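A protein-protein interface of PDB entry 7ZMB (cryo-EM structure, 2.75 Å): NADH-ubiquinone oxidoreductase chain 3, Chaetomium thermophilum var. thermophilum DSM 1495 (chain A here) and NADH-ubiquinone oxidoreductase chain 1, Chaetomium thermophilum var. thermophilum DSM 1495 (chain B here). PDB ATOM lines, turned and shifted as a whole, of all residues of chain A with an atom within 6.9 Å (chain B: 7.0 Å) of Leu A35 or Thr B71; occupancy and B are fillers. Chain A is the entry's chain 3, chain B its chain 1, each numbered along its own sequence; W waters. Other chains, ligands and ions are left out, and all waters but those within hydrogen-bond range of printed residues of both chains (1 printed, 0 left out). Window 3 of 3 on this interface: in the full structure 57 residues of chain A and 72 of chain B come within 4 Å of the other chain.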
ATOM      1  N   HIS A  28     -18.297  -2.664 -14.904  1.00  0.00           N
ATOM      2  CA  HIS A  28     -18.333  -3.397 -13.610  1.00  0.00           C
ATOM      3  C   HIS A  28     -19.780  -3.441 -13.135  1.00  0.00           C
ATOM      4  O   HIS A  28     -20.274  -2.408 -12.663  1.00  0.00           O
ATOM      5  CB  HIS A  28     -17.357  -2.821 -12.579  1.00  0.00           C
ATOM      6  CG  HIS A  28     -17.021  -3.785 -11.494  1.00  0.00           C
ATOM      7  ND1 HIS A  28     -17.492  -3.643 -10.206  1.00  0.00           N
ATOM      8  CD2 HIS A  28     -16.283  -4.915 -11.506  1.00  0.00           C
ATOM      9  CE1 HIS A  28     -17.048  -4.638  -9.467  1.00  0.00           C
ATOM     10  NE2 HIS A  28     -16.303  -5.431 -10.241  1.00  0.00           N
ATOM     11  N   ASN A  29     -20.432  -4.589 -13.283  1.00  0.00           N
ATOM     12  CA  ASN A  29     -21.868  -4.736 -12.948  1.00  0.00           C
ATOM     13  C   ASN A  29     -22.032  -5.966 -12.055  1.00  0.00           C
ATOM     14  O   ASN A  29     -22.495  -7.001 -12.551  1.00  0.00           O
ATOM     15  CB  ASN A  29     -22.688  -4.900 -14.228  1.00  0.00           C
ATOM     16  CG  ASN A  29     -22.408  -3.809 -15.243  1.00  0.00           C
ATOM     17  OD1 ASN A  29     -21.635  -4.007 -16.177  1.00  0.00           O
ATOM     18  ND2 ASN A  29     -23.013  -2.650 -15.053  1.00  0.00           N
ATOM     19  N   PRO A  30     -21.652  -5.899 -10.764  1.00  0.00           N
ATOM     20  CA  PRO A  30     -21.704  -7.073  -9.900  1.00  0.00           C
ATOM     21  C   PRO A  30     -23.103  -7.415  -9.363  1.00  0.00           C
ATOM     22  O   PRO A  30     -23.747  -6.561  -8.790  1.00  0.00           O
ATOM     23  CB  PRO A  30     -20.732  -6.660  -8.786  1.00  0.00           C
ATOM     24  CG  PRO A  30     -20.875  -5.163  -8.677  1.00  0.00           C
ATOM     25  CD  PRO A  30     -21.155  -4.700 -10.088  1.00  0.00           C
ATOM     26  N   TYR A  31     -23.538  -8.663  -9.552  1.00  0.00           N
ATOM     27  CA  TYR A  31     -24.846  -9.088  -8.986  1.00  0.00           C
ATOM     28  C   TYR A  31     -24.701 -10.430  -8.273  1.00  0.00           C
ATOM     29  O   TYR A  31     -23.648 -11.057  -8.428  1.00  0.00           O
ATOM     30  CB  TYR A  31     -26.007  -8.926  -9.971  1.00  0.00           C
ATOM     31  CG  TYR A  31     -25.873  -9.659 -11.275  1.00  0.00           C
ATOM     32  CD1 TYR A  31     -25.330  -9.039 -12.384  1.00  0.00           C
ATOM     33  CD2 TYR A  31     -26.313 -10.963 -11.398  1.00  0.00           C
ATOM     34  CE1 TYR A  31     -25.214  -9.703 -13.591  1.00  0.00           C
ATOM     35  CE2 TYR A  31     -26.202 -11.641 -12.595  1.00  0.00           C
ATOM     36  CZ  TYR A  31     -25.653 -11.007 -13.693  1.00  0.00           C
ATOM     37  OH  TYR A  31     -25.544 -11.669 -14.877  1.00  0.00           O
ATOM     38  N   LYS A  32     -25.751 -10.890  -7.596  1.00  0.00           N
ATOM     39  CA  LYS A  32     -25.649 -12.098  -6.740  1.00  0.00           C
ATOM     40  C   LYS A  32     -25.207 -13.348  -7.502  1.00  0.00           C
ATOM     41  O   LYS A  32     -24.311 -14.042  -7.006  1.00  0.00           O
ATOM     42  CB  LYS A  32     -27.021 -12.373  -6.111  1.00  0.00           C
ATOM     43  CG  LYS A  32     -27.125 -13.645  -5.284  1.00  0.00           C
ATOM     44  CD  LYS A  32     -28.551 -14.025  -4.961  1.00  0.00           C
ATOM     45  CE  LYS A  32     -29.159 -13.188  -3.858  1.00  0.00           C
ATOM     46  NZ  LYS A  32     -28.528 -13.473  -2.548  1.00  0.00           N
ATOM     47  N   GLU A  33     -25.772 -13.626  -8.667  1.00  0.00           N
ATOM     48  CA  GLU A  33     -25.432 -14.917  -9.322  1.00  0.00           C
ATOM     49  C   GLU A  33     -24.081 -14.794 -10.025  1.00  0.00           C
ATOM     50  O   GLU A  33     -23.341 -15.788 -10.031  1.00  0.00           O
ATOM     51  CB  GLU A  33     -26.618 -15.454 -10.117  1.00  0.00           C
ATOM     52  CG  GLU A  33     -27.815 -15.745  -9.237  1.00  0.00           C
ATOM     53  CD  GLU A  33     -27.600 -16.893  -8.266  1.00  0.00           C
ATOM     54  OE1 GLU A  33     -27.503 -18.045  -8.730  1.00  0.00           O
ATOM     55  OE2 GLU A  33     -27.523 -16.631  -7.051  1.00  0.00           O
ATOM     56  N   LYS A  34     -23.775 -13.620 -10.570  1.00  0.00           N
ATOM     57  CA  LYS A  34     -22.431 -13.374 -11.145  1.00  0.00           C
ATOM     58  C   LYS A  34     -21.377 -13.557 -10.058  1.00  0.00           C
ATOM     59  O   LYS A  34     -20.289 -14.035 -10.373  1.00  0.00           O
ATOM     60  CB  LYS A  34     -22.362 -11.962 -11.725  1.00  0.00           C
ATOM     61  CG  LYS A  34     -20.975 -11.489 -12.132  1.00  0.00           C
ATOM     62  CD  LYS A  34     -21.001 -10.234 -12.958  1.00  0.00           C
ATOM     63  CE  LYS A  34     -21.663 -10.441 -14.300  1.00  0.00           C
ATOM     64  NZ  LYS A  34     -21.762  -9.170 -15.050  1.00  0.00           N
ATOM     65  N   LEU A  35     -21.695 -13.213  -8.813  1.00  0.00           N
ATOM     66  CA  LEU A  35     -20.662 -13.274  -7.753  1.00  0.00           C
ATOM     67  C   LEU A  35     -20.699 -14.593  -6.962  1.00  0.00           C
ATOM     68  O   LEU A  35     -20.078 -14.622  -5.908  1.00  0.00           O
ATOM     69  CB  LEU A  35     -20.809 -12.028  -6.877  1.00  0.00           C
ATOM     70  CG  LEU A  35     -19.915 -10.842  -7.236  1.00  0.00           C
ATOM     71  CD1 LEU A  35     -20.068 -10.449  -8.697  1.00  0.00           C
ATOM     72  CD2 LEU A  35     -20.209  -9.655  -6.333  1.00  0.00           C
ATOM     73  N   SER A  36     -21.364 -15.645  -7.458  1.00  0.00           N
ATOM     74  CA  SER A  36     -21.377 -16.919  -6.765  1.00  0.00           C
ATOM     75  C   SER A  36     -20.164 -17.757  -7.155  1.00  0.00           C
ATOM     76  O   SER A  36     -19.465 -17.481  -8.131  1.00  0.00           O
ATOM     77  CB  SER A  36     -22.657 -17.687  -7.072  1.00  0.00           C
ATOM     78  OG  SER A  36     -23.796 -16.869  -6.905  1.00  0.00           O
ATOM     79  N   ALA A  37     -19.910 -18.787  -6.358  1.00  0.00           N
ATOM     80  CA  ALA A  37     -18.882 -19.755  -6.689  1.00  0.00           C
ATOM     81  C   ALA A  37     -19.277 -20.535  -7.930  1.00  0.00           C
ATOM     82  O   ALA A  37     -20.458 -20.781  -8.184  1.00  0.00           O
ATOM     83  CB  ALA A  37     -18.650 -20.717  -5.525  1.00  0.00           C
ATOM     84  N   TYR B  67     -13.893  -7.506 -14.446  1.00  0.00           N
ATOM     85  CA  TYR B  67     -13.327  -8.375 -13.386  1.00  0.00           C
ATOM     86  C   TYR B  67     -14.434  -8.749 -12.421  1.00  0.00           C
ATOM     87  O   TYR B  67     -15.325  -7.955 -12.140  1.00  0.00           O
ATOM     88  CB  TYR B  67     -12.086  -7.785 -12.695  1.00  0.00           C
ATOM     89  CG  TYR B  67     -12.386  -6.700 -11.694  1.00  0.00           C
ATOM     90  CD1 TYR B  67     -12.504  -5.384 -12.096  1.00  0.00           C
ATOM     91  CD2 TYR B  67     -12.576  -6.992 -10.357  1.00  0.00           C
ATOM     92  CE1 TYR B  67     -12.805  -4.380 -11.196  1.00  0.00           C
ATOM     93  CE2 TYR B  67     -12.873  -5.998  -9.442  1.00  0.00           C
ATOM     94  CZ  TYR B  67     -12.980  -4.685  -9.861  1.00  0.00           C
ATOM     95  OH  TYR B  67     -13.268  -3.692  -8.971  1.00  0.00           O
ATOM     96  N   VAL B  68     -14.363  -9.960 -11.928  1.00  0.00           N
ATOM     97  CA  VAL B  68     -15.343 -10.358 -10.896  1.00  0.00           C
ATOM     98  C   VAL B  68     -14.627 -10.723  -9.598  1.00  0.00           C
ATOM     99  O   VAL B  68     -13.630 -11.422  -9.673  1.00  0.00           O
ATOM    100  CB  VAL B  68     -16.232 -11.503 -11.403  1.00  0.00           C
ATOM    101  CG1 VAL B  68     -16.939 -12.246 -10.280  1.00  0.00           C
ATOM    102  CG2 VAL B  68     -17.216 -11.026 -12.453  1.00  0.00           C
ATOM    103  N   GLY B  69     -15.072 -10.181  -8.486  1.00  0.00           N
ATOM    104  CA  GLY B  69     -14.600 -10.579  -7.188  1.00  0.00           C
ATOM    105  C   GLY B  69     -15.634 -11.422  -6.480  1.00  0.00           C
ATOM    106  O   GLY B  69     -16.648 -10.920  -5.991  1.00  0.00           O
ATOM    107  N   PRO B  70     -15.422 -12.765  -6.432  1.00  0.00           N
ATOM    108  CA  PRO B  70     -16.401 -13.663  -5.814  1.00  0.00           C
ATOM    109  C   PRO B  70     -16.677 -13.333  -4.337  1.00  0.00           C
ATOM    110  O   PRO B  70     -15.761 -12.944  -3.638  1.00  0.00           O
ATOM    111  CB  PRO B  70     -15.803 -15.063  -6.027  1.00  0.00           C
ATOM    112  CG  PRO B  70     -14.878 -14.902  -7.191  1.00  0.00           C
ATOM    113  CD  PRO B  70     -14.265 -13.548  -6.928  1.00  0.00           C
ATOM    114  N   THR B  71     -17.914 -13.512  -3.882  1.00  0.00           N
ATOM    115  CA  THR B  71     -18.313 -13.167  -2.490  1.00  0.00           C
ATOM    116  C   THR B  71     -17.642 -14.098  -1.486  1.00  0.00           C
ATOM    117  O   THR B  71     -17.379 -13.660  -0.360  1.00  0.00           O
ATOM    118  CB  THR B  71     -19.828 -13.308  -2.322  1.00  0.00           C
ATOM    119  OG1 THR B  71     -20.157 -14.678  -2.100  1.00  0.00           O
ATOM    120  CG2 THR B  71     -20.580 -12.787  -3.519  1.00  0.00           C
ATOM    121  N   GLN B  72     -17.406 -15.341  -1.882  1.00  0.00           N
ATOM    122  CA  GLN B  72     -16.784 -16.330  -0.975  1.00  0.00           C
ATOM    123  C   GLN B  72     -15.265 -16.173  -0.996  1.00  0.00           C
ATOM    124  O   GLN B  72     -14.631 -16.804  -0.166  1.00  0.00           O
ATOM    125  CB  GLN B  72     -17.218 -17.741  -1.380  1.00  0.00           C
ATOM    126  CG  GLN B  72     -18.719 -17.961  -1.285  1.00  0.00           C
ATOM    127  CD  GLN B  72     -19.259 -17.745   0.107  1.00  0.00           C
ATOM    128  OE1 GLN B  72     -19.503 -16.622   0.537  1.00  0.00           O
ATOM    129  NE2 GLN B  72     -19.467 -18.835   0.824  1.00  0.00           N
ATOM    130  N   ALA B  73     -14.716 -15.365  -1.899  1.00  0.00           N
ATOM    131  CA  ALA B  73     -13.247 -15.241  -2.057  1.00  0.00           C
ATOM    132  C   ALA B  73     -12.583 -14.250  -1.100  1.00  0.00           C
ATOM    133  O   ALA B  73     -13.166 -13.177  -0.874  1.00  0.00           O
ATOM    134  CB  ALA B  73     -12.934 -14.855  -3.479  1.00  0.00           C
ATOM    135  N   ASN B  74     -11.406 -14.598  -0.567  1.00  0.00           N
ATOM    136  CA  ASN B  74     -10.594 -13.638   0.219  1.00  0.00           C
ATOM    137  C   ASN B  74     -10.028 -12.689  -0.841  1.00  0.00           C
ATOM    138  O   ASN B  74      -9.006 -13.058  -1.427  1.00  0.00           O
ATOM    139  CB  ASN B  74      -9.499 -14.387   0.971  1.00  0.00           C
ATOM    140  CG  ASN B  74     -10.025 -14.975   2.255  1.00  0.00           C
ATOM    141  OD1 ASN B  74      -9.735 -16.117   2.595  1.00  0.00           O
ATOM    142  ND2 ASN B  74     -10.831 -14.203   2.961  1.00  0.00           N
ATOM    143  N   LEU B  75     -10.652 -11.533  -1.079  1.00  0.00           N
ATOM    144  CA  LEU B  75     -10.306 -10.638  -2.220  1.00  0.00           C
ATOM    145  C   LEU B  75      -8.911  -9.999  -2.230  1.00  0.00           C
ATOM    146  O   LEU B  75      -8.340  -9.907  -3.326  1.00  0.00           O
ATOM    147  CB  LEU B  75     -11.421  -9.606  -2.398  1.00  0.00           C
ATOM    148  CG  LEU B  75     -12.002  -9.516  -3.808  1.00  0.00           C
ATOM    149  CD1 LEU B  75     -12.464 -10.879  -4.297  1.00  0.00           C
ATOM    150  CD2 LEU B  75     -13.146  -8.517  -3.862  1.00  0.00           C
ATOM    151  N   ALA B 132      -9.785 -18.211  -3.905  1.00  0.00           N
ATOM    152  CA  ALA B 132     -11.037 -18.194  -4.652  1.00  0.00           C
ATOM    153  C   ALA B 132     -12.181 -18.805  -3.859  1.00  0.00           C
ATOM    154  O   ALA B 132     -13.333 -18.391  -4.018  1.00  0.00           O
ATOM    155  CB  ALA B 132     -10.858 -18.936  -5.970  1.00  0.00           C
ATOM    156  N   ASN B 133     -11.887 -19.781  -3.007  1.00  0.00           N
ATOM    157  CA  ASN B 133     -12.895 -20.442  -2.189  1.00  0.00           C
ATOM    158  C   ASN B 133     -13.970 -21.091  -3.063  1.00  0.00           C
ATOM    159  O   ASN B 133     -15.163 -21.029  -2.769  1.00  0.00           O
ATOM    160  CB  ASN B 133     -13.500 -19.465  -1.179  1.00  0.00           C
ATOM    161  CG  ASN B 133     -14.184 -20.160  -0.038  1.00  0.00           C
ATOM    162  OD1 ASN B 133     -14.633 -21.291  -0.164  1.00  0.00           O
ATOM    163  ND2 ASN B 133     -14.276 -19.480   1.090  1.00  0.00           N
ATOM    164  N   GLU B 223     -11.934 -19.123 -11.148  1.00  0.00           N
ATOM    165  CA  GLU B 223     -12.694 -17.898 -10.776  1.00  0.00           C
ATOM    166  C   GLU B 223     -12.043 -16.644 -11.370  1.00  0.00           C
ATOM    167  O   GLU B 223     -12.705 -15.599 -11.355  1.00  0.00           O
ATOM    168  CB  GLU B 223     -12.895 -17.772  -9.258  1.00  0.00           C
ATOM    169  CG  GLU B 223     -13.965 -18.656  -8.647  1.00  0.00           C
ATOM    170  CD  GLU B 223     -15.397 -18.578  -9.157  1.00  0.00           C
ATOM    171  OE1 GLU B 223     -15.610 -18.649 -10.381  1.00  0.00           O
ATOM    172  OE2 GLU B 223     -16.306 -18.476  -8.315  1.00  0.00           O
HETATM  173  O   HOH W   1     -18.572 -15.922  -4.505  1.00  0.00           O
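O of Tyr B67 lies close to NE2 of His A28 (3.3 Å).
The backbone NH of Thr B71 lies close to the backbone carbonyl oxygen of Leu A35, 3.2 Å away.
The side-chain carboxylate (OE2) of Glu B223 lies close to the backbone carbonyl oxygen (O) of Ser A36.
Water W1 lies within hydrogen-bond range of O of Leu A35 (2.4 Å), N of Thr B71 (2.6 Å) and N of Gln B72 (2.9 Å).
Hydrophobic or aromatic side chains of chain A that line the printed part of chain B: His A28 and Leu A35.
Among the printed residues, 8 pairs touch across the chains.
Among the printed residues, no Asp or Glu carboxylate lies within 4 Å of a Lys or Arg side-chain nitrogen of the other chain.
Among the printed residues, pairs that only touch across the chains: Lys A34 with Val B68 (3.8 Å), Leu A35 with Val B68 (3.9 Å), Leu A35 with Gly B69 (3.5 Å), Leu A35 with Pro B70 (3.8 Å) and Ala A37 with Glu B223 (3.3 Å).
Thr B71 touches just one residue of chain A: Leu A35.
Of the printed residues of chain A, Tyr B67 touches His A28 (3.2 Å).
Printed residues of chain B within 4 Å of His A28: Tyr B67 (3.2 Å).
Of the printed residues of chain B, Lys A34 touches Val B68 (3.8 Å).
Of the printed residues of chain B, Ala A37 touches Glu B223.
Printed residues of chain A within 4 Å of Pro B70: Leu A35.
Pro A30 touches none of the printed residues of chain B.
Asn B133 touches none of the printed residues of chain A.
The nearest residue of chain B that does not touch Leu A35 is Gln B72 (4.9 Å).
OE1 of Gln B72 sits at hydrogen-bond distance from OG1 of Thr B71 (3.3 Å).
The backbone carbonyl oxygen (O) of Asn A29 is in hydrogen-bond range of the side-chain amino group (NZ) of Lys A34 (3.4 Å).
OG of Ser A36 sits at hydrogen-bond distance from O of Lys A32 (2.9 Å).
The backbone carbonyl oxygen of Glu A33 sits at hydrogen-bond distance from the side-chain hydroxyl of Ser A36, at 3.3 Å.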
